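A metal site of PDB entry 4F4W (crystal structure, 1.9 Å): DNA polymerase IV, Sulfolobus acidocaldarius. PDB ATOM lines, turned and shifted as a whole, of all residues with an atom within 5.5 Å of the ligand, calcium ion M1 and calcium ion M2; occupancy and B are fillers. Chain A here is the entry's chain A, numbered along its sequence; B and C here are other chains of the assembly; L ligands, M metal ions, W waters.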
ATOM      1  N   ASP A   7      19.219  15.777 -14.257  1.00  0.00           N
ATOM      2  CA  ASP A   7      18.918  14.481 -13.678  1.00  0.00           C
ATOM      3  C   ASP A   7      20.159  14.046 -12.901  1.00  0.00           C
ATOM      4  O   ASP A   7      21.242  13.927 -13.486  1.00  0.00           O
ATOM      5  CB  ASP A   7      18.592  13.501 -14.782  1.00  0.00           C
ATOM      6  CG  ASP A   7      18.022  12.184 -14.264  1.00  0.00           C
ATOM      7  OD1 ASP A   7      17.090  11.631 -14.881  1.00  0.00           O
ATOM      8  OD2 ASP A   7      18.524  11.679 -13.287  1.00  0.00           O
ATOM      9  N   PHE A   8      20.040  13.868 -11.579  1.00  0.00           N
ATOM     10  CA  PHE A   8      21.231  13.677 -10.738  1.00  0.00           C
ATOM     11  C   PHE A   8      21.810  12.266 -10.983  1.00  0.00           C
ATOM     12  O   PHE A   8      21.069  11.314 -11.081  1.00  0.00           O
ATOM     13  CB  PHE A   8      20.917  13.853  -9.239  1.00  0.00           C
ATOM     14  CG  PHE A   8      20.197  15.139  -8.895  1.00  0.00           C
ATOM     15  CD1 PHE A   8      19.413  15.214  -7.746  1.00  0.00           C
ATOM     16  CD2 PHE A   8      20.280  16.247  -9.694  1.00  0.00           C
ATOM     17  CE1 PHE A   8      18.729  16.378  -7.414  1.00  0.00           C
ATOM     18  CE2 PHE A   8      19.603  17.423  -9.361  1.00  0.00           C
ATOM     19  CZ  PHE A   8      18.827  17.477  -8.220  1.00  0.00           C
ATOM     20  N   ASP A   9      23.132  12.094 -11.063  1.00  0.00           N
ATOM     21  CA  ASP A   9      23.641  10.744 -11.345  1.00  0.00           C
ATOM     22  C   ASP A   9      23.526   9.796 -10.135  1.00  0.00           C
ATOM     23  O   ASP A   9      23.872  10.173  -9.028  1.00  0.00           O
ATOM     24  CB  ASP A   9      25.117  10.784 -11.784  1.00  0.00           C
ATOM     25  CG  ASP A   9      25.336  11.563 -13.065  1.00  0.00           C
ATOM     26  OD1 ASP A   9      26.436  12.146 -13.203  1.00  0.00           O
ATOM     27  OD2 ASP A   9      24.410  11.607 -13.909  1.00  0.00           O
ATOM     28  N   TYR A  10      23.071   8.558 -10.386  1.00  0.00           N
ATOM     29  CA  TYR A  10      22.968   7.462  -9.386  1.00  0.00           C
ATOM     30  C   TYR A  10      22.659   7.998  -8.004  1.00  0.00           C
ATOM     31  O   TYR A  10      23.381   7.740  -7.008  1.00  0.00           O
ATOM     32  CB  TYR A  10      24.192   6.508  -9.409  1.00  0.00           C
ATOM     33  CG  TYR A  10      25.563   7.074  -9.020  1.00  0.00           C
ATOM     34  CD1 TYR A  10      26.159   6.735  -7.819  1.00  0.00           C
ATOM     35  CD2 TYR A  10      26.276   7.887  -9.898  1.00  0.00           C
ATOM     36  CE1 TYR A  10      27.438   7.227  -7.479  1.00  0.00           C
ATOM     37  CE2 TYR A  10      27.532   8.402  -9.554  1.00  0.00           C
ATOM     38  CZ  TYR A  10      28.093   8.068  -8.354  1.00  0.00           C
ATOM     39  OH  TYR A  10      29.339   8.540  -8.032  1.00  0.00           O
ATOM     40  N   PHE A  11      21.577   8.789  -7.955  1.00  0.00           N
ATOM     41  CA  PHE A  11      21.430   9.797  -6.899  1.00  0.00           C
ATOM     42  C   PHE A  11      21.646   9.324  -5.458  1.00  0.00           C
ATOM     43  O   PHE A  11      22.560   9.826  -4.764  1.00  0.00           O
ATOM     44  CB  PHE A  11      20.114  10.566  -7.045  1.00  0.00           C
ATOM     45  CG  PHE A  11      19.979  11.703  -6.069  1.00  0.00           C
ATOM     46  CD1 PHE A  11      21.046  12.590  -5.843  1.00  0.00           C
ATOM     47  CD2 PHE A  11      18.779  11.915  -5.398  1.00  0.00           C
ATOM     48  CE1 PHE A  11      20.915  13.636  -4.929  1.00  0.00           C
ATOM     49  CE2 PHE A  11      18.651  12.976  -4.496  1.00  0.00           C
ATOM     50  CZ  PHE A  11      19.715  13.831  -4.262  1.00  0.00           C
ATOM     51  N   PHE A  12      20.847   8.373  -4.977  1.00  0.00           N
ATOM     52  CA  PHE A  12      20.944   8.017  -3.565  1.00  0.00           C
ATOM     53  C   PHE A  12      22.324   7.449  -3.221  1.00  0.00           C
ATOM     54  O   PHE A  12      22.864   7.741  -2.155  1.00  0.00           O
ATOM     55  CB  PHE A  12      19.884   6.980  -3.126  1.00  0.00           C
ATOM     56  CG  PHE A  12      18.465   7.452  -3.197  1.00  0.00           C
ATOM     57  CD1 PHE A  12      18.108   8.724  -3.646  1.00  0.00           C
ATOM     58  CD2 PHE A  12      17.455   6.578  -2.803  1.00  0.00           C
ATOM     59  CE1 PHE A  12      16.797   9.105  -3.723  1.00  0.00           C
ATOM     60  CE2 PHE A  12      16.158   6.957  -2.847  1.00  0.00           C
ATOM     61  CZ  PHE A  12      15.799   8.222  -3.320  1.00  0.00           C
ATOM     62  N   ALA A  13      22.889   6.624  -4.110  1.00  0.00           N
ATOM     63  CA  ALA A  13      24.208   6.048  -3.855  1.00  0.00           C
ATOM     64  C   ALA A  13      25.283   7.132  -3.881  1.00  0.00           C
ATOM     65  O   ALA A  13      26.219   7.100  -3.083  1.00  0.00           O
ATOM     66  CB  ALA A  13      24.549   4.919  -4.883  1.00  0.00           C
ATOM     67  N   VAL A  43      16.417  -3.113  -3.858  1.00  0.00           N
ATOM     68  CA  VAL A  43      17.466  -2.136  -4.117  1.00  0.00           C
ATOM     69  C   VAL A  43      16.806  -0.858  -4.601  1.00  0.00           C
ATOM     70  O   VAL A  43      16.013  -0.900  -5.533  1.00  0.00           O
ATOM     71  CB  VAL A  43      18.391  -2.640  -5.230  1.00  0.00           C
ATOM     72  CG1 VAL A  43      19.342  -1.535  -5.692  1.00  0.00           C
ATOM     73  CG2 VAL A  43      19.166  -3.856  -4.739  1.00  0.00           C
ATOM     74  N   ALA A  44      17.149   0.257  -3.966  1.00  0.00           N
ATOM     75  CA  ALA A  44      16.703   1.585  -4.432  1.00  0.00           C
ATOM     76  C   ALA A  44      17.607   2.059  -5.567  1.00  0.00           C
ATOM     77  O   ALA A  44      17.138   2.578  -6.598  1.00  0.00           O
ATOM     78  CB  ALA A  44      16.724   2.626  -3.279  1.00  0.00           C
ATOM     79  N   THR A  45      18.916   1.924  -5.381  1.00  0.00           N
ATOM     80  CA  THR A  45      19.813   2.201  -6.471  1.00  0.00           C
ATOM     81  C   THR A  45      21.196   1.691  -6.167  1.00  0.00           C
ATOM     82  O   THR A  45      21.520   1.372  -5.007  1.00  0.00           O
ATOM     83  CB  THR A  45      19.817   3.662  -6.825  1.00  0.00           C
ATOM     84  OG1 THR A  45      20.310   3.834  -8.174  1.00  0.00           O
ATOM     85  CG2 THR A  45      20.665   4.442  -5.855  1.00  0.00           C
ATOM     86  N   ALA A  46      21.995   1.603  -7.217  1.00  0.00           N
ATOM     87  CA  ALA A  46      23.376   1.134  -7.071  1.00  0.00           C
ATOM     88  C   ALA A  46      24.257   2.089  -7.831  1.00  0.00           C
ATOM     89  O   ALA A  46      23.827   2.657  -8.840  1.00  0.00           O
ATOM     90  CB  ALA A  46      23.521  -0.251  -7.645  1.00  0.00           C
ATOM     91  N   TYR A  48      27.535   2.938 -10.328  1.00  0.00           N
ATOM     92  CA  TYR A  48      27.809   2.320 -11.627  1.00  0.00           C
ATOM     93  C   TYR A  48      28.696   1.076 -11.495  1.00  0.00           C
ATOM     94  O   TYR A  48      28.520   0.121 -12.244  1.00  0.00           O
ATOM     95  CB  TYR A  48      28.400   3.354 -12.585  1.00  0.00           C
ATOM     96  CG  TYR A  48      27.491   4.556 -12.789  1.00  0.00           C
ATOM     97  CD1 TYR A  48      26.122   4.400 -12.897  1.00  0.00           C
ATOM     98  CD2 TYR A  48      28.007   5.844 -12.813  1.00  0.00           C
ATOM     99  CE1 TYR A  48      25.284   5.491 -13.077  1.00  0.00           C
ATOM    100  CE2 TYR A  48      27.183   6.935 -12.990  1.00  0.00           C
ATOM    101  CZ  TYR A  48      25.817   6.736 -13.118  1.00  0.00           C
ATOM    102  OH  TYR A  48      24.985   7.832 -13.291  1.00  0.00           O
ATOM    103  N   ARG A  51      26.388  -1.640 -10.761  1.00  0.00           N
ATOM    104  CA  ARG A  51      25.602  -1.959 -11.935  1.00  0.00           C
ATOM    105  C   ARG A  51      26.382  -2.853 -12.921  1.00  0.00           C
ATOM    106  O   ARG A  51      25.818  -3.705 -13.607  1.00  0.00           O
ATOM    107  CB  ARG A  51      25.112  -0.684 -12.638  1.00  0.00           C
ATOM    108  CG  ARG A  51      24.038   0.068 -11.850  1.00  0.00           C
ATOM    109  CD  ARG A  51      23.611   1.319 -12.548  1.00  0.00           C
ATOM    110  NE  ARG A  51      23.057   2.276 -11.592  1.00  0.00           N
ATOM    111  CZ  ARG A  51      22.428   3.386 -11.936  1.00  0.00           C
ATOM    112  NH1 ARG A  51      22.287   3.681 -13.210  1.00  0.00           N
ATOM    113  NH2 ARG A  51      21.930   4.192 -10.990  1.00  0.00           N
ATOM    114  N   ALA A  57      18.160  -1.317  -9.842  1.00  0.00           N
ATOM    115  CA  ALA A  57      17.106  -0.772  -8.967  1.00  0.00           C
ATOM    116  C   ALA A  57      15.890  -1.681  -9.033  1.00  0.00           C
ATOM    117  O   ALA A  57      15.534  -2.145 -10.105  1.00  0.00           O
ATOM    118  CB  ALA A  57      16.715   0.645  -9.406  1.00  0.00           C
ATOM    119  N   GLY A  58      15.250  -1.911  -7.887  1.00  0.00           N
ATOM    120  CA  GLY A  58      14.026  -2.696  -7.835  1.00  0.00           C
ATOM    121  C   GLY A  58      14.295  -4.156  -7.543  1.00  0.00           C
ATOM    122  O   GLY A  58      13.407  -4.914  -7.168  1.00  0.00           O
ATOM    123  N   MET A  76      18.675   2.707   3.073  1.00  0.00           N
ATOM    124  CA  MET A  76      18.244   3.948   2.458  1.00  0.00           C
ATOM    125  C   MET A  76      18.074   4.984   3.589  1.00  0.00           C
ATOM    126  O   MET A  76      17.517   4.673   4.641  1.00  0.00           O
ATOM    127  CB  MET A  76      16.933   3.670   1.685  1.00  0.00           C
ATOM    128  CG  MET A  76      16.624   4.661   0.535  1.00  0.00           C
ATOM    129  SD  MET A  76      14.920   4.681   0.016  1.00  0.00           S
ATOM    130  CE  MET A  76      14.030   4.198   1.527  1.00  0.00           C
ATOM    131  N   SER A 103      10.775  15.211  -9.839  1.00  0.00           N
ATOM    132  CA  SER A 103      10.949  14.098  -8.921  1.00  0.00           C
ATOM    133  C   SER A 103      12.049  14.498  -7.954  1.00  0.00           C
ATOM    134  O   SER A 103      12.567  15.596  -8.050  1.00  0.00           O
ATOM    135  CB  SER A 103      11.329  12.781  -9.641  1.00  0.00           C
ATOM    136  OG  SER A 103      12.710  12.675  -9.963  1.00  0.00           O
ATOM    137  N   ILE A 104      12.393  13.620  -7.026  1.00  0.00           N
ATOM    138  CA  ILE A 104      13.448  13.931  -6.067  1.00  0.00           C
ATOM    139  C   ILE A 104      14.793  14.204  -6.749  1.00  0.00           C
ATOM    140  O   ILE A 104      15.703  14.805  -6.158  1.00  0.00           O
ATOM    141  CB  ILE A 104      13.615  12.784  -5.047  1.00  0.00           C
ATOM    142  CG1 ILE A 104      14.519  13.264  -3.903  1.00  0.00           C
ATOM    143  CG2 ILE A 104      14.114  11.500  -5.715  1.00  0.00           C
ATOM    144  CD1 ILE A 104      14.603  12.296  -2.779  1.00  0.00           C
ATOM    145  N   ASP A 105      14.982  13.735  -7.966  1.00  0.00           N
ATOM    146  CA  ASP A 105      16.280  14.008  -8.563  1.00  0.00           C
ATOM    147  C   ASP A 105      16.281  14.545  -9.969  1.00  0.00           C
ATOM    148  O   ASP A 105      17.305  14.467 -10.647  1.00  0.00           O
ATOM    149  CB  ASP A 105      17.213  12.813  -8.472  1.00  0.00           C
ATOM    150  CG  ASP A 105      17.035  11.860  -9.619  1.00  0.00           C
ATOM    151  OD1 ASP A 105      15.920  11.748 -10.140  1.00  0.00           O
ATOM    152  OD2 ASP A 105      18.010  11.199  -9.968  1.00  0.00           O
ATOM    153  N   GLU A 106      15.167  15.128 -10.407  1.00  0.00           N
ATOM    154  CA  GLU A 106      15.209  15.760 -11.718  1.00  0.00           C
ATOM    155  C   GLU A 106      14.282  16.970 -11.838  1.00  0.00           C
ATOM    156  O   GLU A 106      13.216  17.049 -11.169  1.00  0.00           O
ATOM    157  CB  GLU A 106      14.980  14.720 -12.809  1.00  0.00           C
ATOM    158  CG  GLU A 106      13.617  14.193 -12.891  1.00  0.00           C
ATOM    159  CD  GLU A 106      13.485  13.012 -13.843  1.00  0.00           C
ATOM    160  OE1 GLU A 106      14.196  12.017 -13.704  1.00  0.00           O
ATOM    161  OE2 GLU A 106      12.666  13.076 -14.748  1.00  0.00           O
ATOM    162  N   LYS A 153      15.002  15.701 -21.957  1.00  0.00           N
ATOM    163  CA  LYS A 153      15.128  14.450 -21.203  1.00  0.00           C
ATOM    164  C   LYS A 153      15.787  13.365 -22.020  1.00  0.00           C
ATOM    165  O   LYS A 153      16.715  12.713 -21.568  1.00  0.00           O
ATOM    166  CB  LYS A 153      13.763  13.964 -20.691  1.00  0.00           C
ATOM    167  CG  LYS A 153      13.827  12.674 -19.887  1.00  0.00           C
ATOM    168  CD  LYS A 153      12.448  12.362 -19.357  1.00  0.00           C
ATOM    169  CE  LYS A 153      12.477  11.275 -18.330  1.00  0.00           C
ATOM    170  NZ  LYS A 153      12.957  11.844 -17.051  1.00  0.00           N
ATOM    171  N   LYS A 160      24.224  10.056 -20.097  1.00  0.00           N
ATOM    172  CA  LYS A 160      24.611   9.655 -18.733  1.00  0.00           C
ATOM    173  C   LYS A 160      25.858   8.788 -18.788  1.00  0.00           C
ATOM    174  O   LYS A 160      26.047   8.032 -19.732  1.00  0.00           O
ATOM    175  CB  LYS A 160      23.495   8.866 -18.036  1.00  0.00           C
ATOM    176  CG  LYS A 160      22.234   9.647 -17.722  1.00  0.00           C
ATOM    177  CD  LYS A 160      21.284   8.867 -16.749  1.00  0.00           C
ATOM    178  CE  LYS A 160      19.957   9.608 -16.469  1.00  0.00           C
ATOM    179  NZ  LYS A 160      18.886   8.821 -15.710  1.00  0.00           N
ATOM    180  P    DG B   5      10.064  -7.046   0.864  1.00  0.00           P
ATOM    181  OP1  DG B   5      10.379  -7.633   2.206  1.00  0.00           O
ATOM    182  OP2  DG B   5       8.703  -7.177   0.276  1.00  0.00           O
ATOM    183  O5'  DG B   5      10.550  -5.539   1.005  1.00  0.00           O
ATOM    184  C5'  DG B   5      10.664  -4.726  -0.147  1.00  0.00           C
ATOM    185  C4'  DG B   5      10.928  -3.333   0.376  1.00  0.00           C
ATOM    186  O4'  DG B   5      11.336  -2.455  -0.689  1.00  0.00           O
ATOM    187  C3'  DG B   5       9.654  -2.688   0.936  1.00  0.00           C
ATOM    188  O3'  DG B   5      10.038  -1.799   1.960  1.00  0.00           O
ATOM    189  C2'  DG B   5       9.062  -2.025  -0.316  1.00  0.00           C
ATOM    190  C1'  DG B   5      10.325  -1.445  -0.946  1.00  0.00           C
ATOM    191  N9   DG B   5      10.406  -1.404  -2.413  1.00  0.00           N
ATOM    192  C8   DG B   5      10.022  -2.374  -3.311  1.00  0.00           C
ATOM    193  N7   DG B   5      10.336  -2.063  -4.550  1.00  0.00           N
ATOM    194  C5   DG B   5      10.979  -0.827  -4.431  1.00  0.00           C
ATOM    195  C6   DG B   5      11.584  -0.009  -5.409  1.00  0.00           C
ATOM    196  O6   DG B   5      11.643  -0.223  -6.633  1.00  0.00           O
ATOM    197  N1   DG B   5      12.158   1.151  -4.871  1.00  0.00           N
ATOM    198  C2   DG B   5      12.166   1.477  -3.542  1.00  0.00           C
ATOM    199  N2   DG B   5      12.771   2.641  -3.152  1.00  0.00           N
ATOM    200  N3   DG B   5      11.627   0.696  -2.630  1.00  0.00           N
ATOM    201  C4   DG B   5      11.061  -0.437  -3.132  1.00  0.00           C
ATOM    202  P    DG B   6       8.959  -1.195   2.996  1.00  0.00           P
ATOM    203  OP1  DG B   6       9.679  -0.856   4.244  1.00  0.00           O
ATOM    204  OP2  DG B   6       7.761  -2.067   2.948  1.00  0.00           O
ATOM    205  O5'  DG B   6       8.571   0.182   2.301  1.00  0.00           O
ATOM    206  C5'  DG B   6       9.573   1.148   2.193  1.00  0.00           C
ATOM    207  C4'  DG B   6       9.099   2.286   1.328  1.00  0.00           C
ATOM    208  O4'  DG B   6       9.228   1.903  -0.039  1.00  0.00           O
ATOM    209  C3'  DG B   6       7.615   2.687   1.521  1.00  0.00           C
ATOM    210  O3'  DG B   6       7.683   4.105   1.610  1.00  0.00           O
ATOM    211  C2'  DG B   6       6.983   2.231   0.184  1.00  0.00           C
ATOM    212  C1'  DG B   6       8.182   2.457  -0.768  1.00  0.00           C
ATOM    213  N9   DG B   6       8.112   1.827  -2.085  1.00  0.00           N
ATOM    214  C8   DG B   6       7.531   0.638  -2.420  1.00  0.00           C
ATOM    215  N7   DG B   6       7.591   0.358  -3.692  1.00  0.00           N
ATOM    216  C5   DG B   6       8.273   1.425  -4.219  1.00  0.00           C
ATOM    217  C6   DG B   6       8.647   1.669  -5.540  1.00  0.00           C
ATOM    218  O6   DG B   6       8.392   0.945  -6.474  1.00  0.00           O
ATOM    219  N1   DG B   6       9.314   2.887  -5.710  1.00  0.00           N
ATOM    220  C2   DG B   6       9.607   3.742  -4.703  1.00  0.00           C
ATOM    221  N2   DG B   6      10.248   4.874  -5.031  1.00  0.00           N
ATOM    222  N3   DG B   6       9.263   3.499  -3.452  1.00  0.00           N
ATOM    223  C4   DG B   6       8.587   2.344  -3.272  1.00  0.00           C
ATOM    224  P    DC C  13      11.297   7.210 -15.309  1.00  0.00           P
ATOM    225  OP1  DC C  13      11.349   8.553 -15.939  1.00  0.00           O
ATOM    226  OP2  DC C  13      12.064   6.018 -15.799  1.00  0.00           O
ATOM    227  O5'  DC C  13      11.724   7.484 -13.780  1.00  0.00           O
ATOM    228  C5'  DC C  13      11.287   8.680 -13.109  1.00  0.00           C
ATOM    229  C4'  DC C  13      11.589   8.444 -11.629  1.00  0.00           C
ATOM    230  O4'  DC C  13      10.919   7.233 -11.211  1.00  0.00           O
ATOM    231  C3'  DC C  13      13.049   8.133 -11.461  1.00  0.00           C
ATOM    232  O3'  DC C  13      13.759   9.345 -11.148  1.00  0.00           O
ATOM    233  C2'  DC C  13      13.107   6.996 -10.441  1.00  0.00           C
ATOM    234  C1'  DC C  13      11.645   6.752 -10.088  1.00  0.00           C
ATOM    235  N1   DC C  13      11.164   5.347  -9.798  1.00  0.00           N
ATOM    236  C2   DC C  13      10.690   4.974  -8.499  1.00  0.00           C
ATOM    237  O2   DC C  13      10.720   5.804  -7.586  1.00  0.00           O
ATOM    238  N3   DC C  13      10.267   3.712  -8.291  1.00  0.00           N
ATOM    239  C4   DC C  13      10.252   2.826  -9.285  1.00  0.00           C
ATOM    240  N4   DC C  13       9.807   1.587  -9.072  1.00  0.00           N
ATOM    241  C5   DC C  13      10.721   3.178 -10.596  1.00  0.00           C
ATOM    242  C6   DC C  13      11.147   4.429 -10.784  1.00  0.00           C
HETATM  243  N1  LIG L   1      14.667   5.061  -6.990  1.00  0.00           N
HETATM  244  C1  LIG L   1      14.052   4.166  -6.173  1.00  0.00           C
HETATM  245  N2  LIG L   1      13.531   3.019  -6.617  1.00  0.00           N
HETATM  246  C2  LIG L   1      13.657   2.733  -7.928  1.00  0.00           C
HETATM  247  C3  LIG L   1      14.292   3.603  -8.804  1.00  0.00           C
HETATM  248  C4  LIG L   1      14.826   4.799  -8.313  1.00  0.00           C
HETATM  249  O1  LIG L   1      13.961   4.428  -4.865  1.00  0.00           O
HETATM  250  N3  LIG L   1      13.133   1.510  -8.468  1.00  0.00           N
HETATM  251  C5  LIG L   1      15.269   6.288  -6.476  1.00  0.00           C
HETATM  252  C6  LIG L   1      16.724   6.063  -6.269  1.00  0.00           C
HETATM  253  C7  LIG L   1      17.356   6.772  -7.422  1.00  0.00           C
HETATM  254  C8  LIG L   1      16.446   7.859  -7.640  1.00  0.00           C
HETATM  255  O2  LIG L   1      15.131   7.307  -7.437  1.00  0.00           O
HETATM  256  O3  LIG L   1      18.697   7.198  -7.182  1.00  0.00           O
HETATM  257  C9  LIG L   1      16.542   8.361  -9.018  1.00  0.00           C
HETATM  258  O4  LIG L   1      16.194   7.397  -9.980  1.00  0.00           O
HETATM  259  P1  LIG L   1      16.895   7.327 -11.384  1.00  0.00           P
HETATM  260  O5  LIG L   1      16.010   6.560 -12.316  1.00  0.00           O
HETATM  261  O6  LIG L   1      17.081   8.675 -11.927  1.00  0.00           O
HETATM  262  O7  LIG L   1      18.260   6.569 -11.228  1.00  0.00           O
HETATM  263  P2  LIG L   1      19.621   6.988 -10.575  1.00  0.00           P
HETATM  264  O8  LIG L   1      19.728   8.401 -10.193  1.00  0.00           O
HETATM  265  O9  LIG L   1      19.838   6.158  -9.347  1.00  0.00           O
HETATM  266  O10 LIG L   1      20.730   6.550 -11.625  1.00  0.00           O
HETATM  267  P3  LIG L   1      20.967   7.290 -13.029  1.00  0.00           P
HETATM  268  O11 LIG L   1      22.391   7.773 -13.002  1.00  0.00           O
HETATM  269  O12 LIG L   1      20.876   6.220 -14.059  1.00  0.00           O
HETATM  270  O13 LIG L   1      19.974   8.439 -13.288  1.00  0.00           O
HETATM  271 CA    CA M   1      19.130  10.107 -11.801  1.00  0.00          CA
HETATM  272 CA    CA M   2      15.768  10.493 -12.676  1.00  0.00          CA
HETATM  273  O   HOH W   1      21.425  10.824 -14.109  1.00  0.00           O
HETATM  274  O   HOH W   2      16.280   3.671 -11.518  1.00  0.00           O
HETATM  275  O   HOH W   3      22.436   5.622 -16.268  1.00  0.00           O
HETATM  276  O   HOH W   4      13.318   0.767 -11.302  1.00  0.00           O
HETATM  277  O   HOH W   5      12.741   6.146  -3.200  1.00  0.00           O
HETATM  278  O   HOH W   6      18.829   4.330 -14.761  1.00  0.00           O
HETATM  279  O   HOH W   7      18.028   3.620  -9.234  1.00  0.00           O
HETATM  280  O   HOH W   8      15.382   9.164 -14.255  1.00  0.00           O
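Within 4 Å of calcium ion M1: Asp 7, Phe 8 and Asp 105. Along chain A the residues within 4 Å of calcium ion M1 span positions 7 to 105.
The side-chain hydroxyl of Tyr 48 sits at hydrogen-bond distance from an oxygen (O11) of the ligand (2.6 Å). O9 of the ligand is in hydrogen-bond range of OG1 of Thr 45 (2.6 Å). The side-chain amino group (NZ) of Lys 160 is in salt-bridge range of an oxygen (O12) of the ligand (3.7 Å). The guanidinium group (NH1) of Arg 51 lies within salt-bridge range of an oxygen (O12) of the ligand, at 3.0 Å. O6 of DG 5 of chain B is in hydrogen-bond range of N3 of the ligand, 2.9 Å away. N4 of DC 13 of chain C sits close to N3 of the ligand, 3.4 Å away. N of Tyr 10 lies within hydrogen-bond range of O11 of the ligand, at 2.8 Å. The backbone NH (N) of Phe 11 lies within hydrogen-bond range of an oxygen (O3) of the ligand (3.4 Å). The backbone NH (N) of Phe 12 lies within hydrogen-bond range of an oxygen (O3) of the ligand, at 3.3 Å.
OD2 of Asp 7 binds calcium ion M1. O13 of the ligand binds calcium ion M1. O of Phe 8 is bound to calcium ion M1 (2.4 Å). The side-chain carboxylate (OD2) of Asp 105 is bound to calcium ion M1 (2.4 Å). Calcium ion M1 is bound by O8 of the ligand, 2.4 Å away. O6 of the ligand binds calcium ion M1 (2.5 Å).
Four residues have an atom within 4 Å of calcium ion M2: Asp 7, Asp 105, Glu 106 and DC 13 of chain C. The nearest printed residue that does not touch calcium ion M2 is Ser 103 (4.6 Å).
Water W8 binds calcium ion M2 (2.1 Å). O6 of the ligand binds calcium ion M2 (2.4 Å). OE1 of Glu 106 binds calcium ion M2, 2.4 Å away. O3' of DC 13 of chain C binds calcium ion M2 (2.8 Å). Calcium ion M2 is bound by the side-chain carboxylate (OD1) of Asp 7. The side-chain carboxylate (OD1) of Asp 105 binds calcium ion M2, 2.8 Å away. Slightly farther from calcium ion M2 lies OD2 of Asp 7 (3.1 Å).
The side-chain amino group (NZ) of Lys 160 lies close to the side-chain carboxylate (OD1) of Asp 7. The side-chain hydroxyl (OG) of Ser 103 sits close to the backbone NH (N) of Asp 105. The side-chain carboxylate of Glu 106 is in salt-bridge range of the side-chain amino group of Lys 153, 2.6 Å away. The side-chain hydroxyl of Thr 45 lies within hydrogen-bond range of the guanidinium group of Arg 51. The backbone carbonyl oxygen of Ala 46 is in hydrogen-bond range of the guanidinium group of Arg 51, 2.9 Å away. NZ of Lys 153 lies within salt-bridge range of OP1 of DC 13 of chain C.
Merely in contact with the ligand: Asp 9 (3.6 Å), Ala 44 (3.5 Å), Ala 57 (3.8 Å) and DG 6 of chain B (3.7 Å). Hydrophobic or aromatic side chains that line the ligand: Phe 11, Phe 12, Ala 44, Tyr 48 and Ala 57. Within 4 Å of the ligand: Asp 7, Phe 8, Asp 9, Tyr 10, Phe 11, Phe 12, Ala 44, Thr 45, Tyr 48, Arg 51, Ala 57, Asp 105, Lys 160, DG 5 of chain B, DG 6 of chain B and DC 13 of chain C.
Water W5 bridges O1 of the ligand (2.7 Å) and N2 of DG 6 of chain B (3.3 Å). Water W1 lies within hydrogen-bond range of the side-chain carboxylate of Asp 9 (3.1 Å), the backbone carbonyl oxygen of Asp 7 (3.2 Å) and an oxygen (O11) of the ligand (3.4 Å). Water W7 lies within hydrogen-bond range of OG1 of Thr 45, O of Ala 44 and O9 of the ligand.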
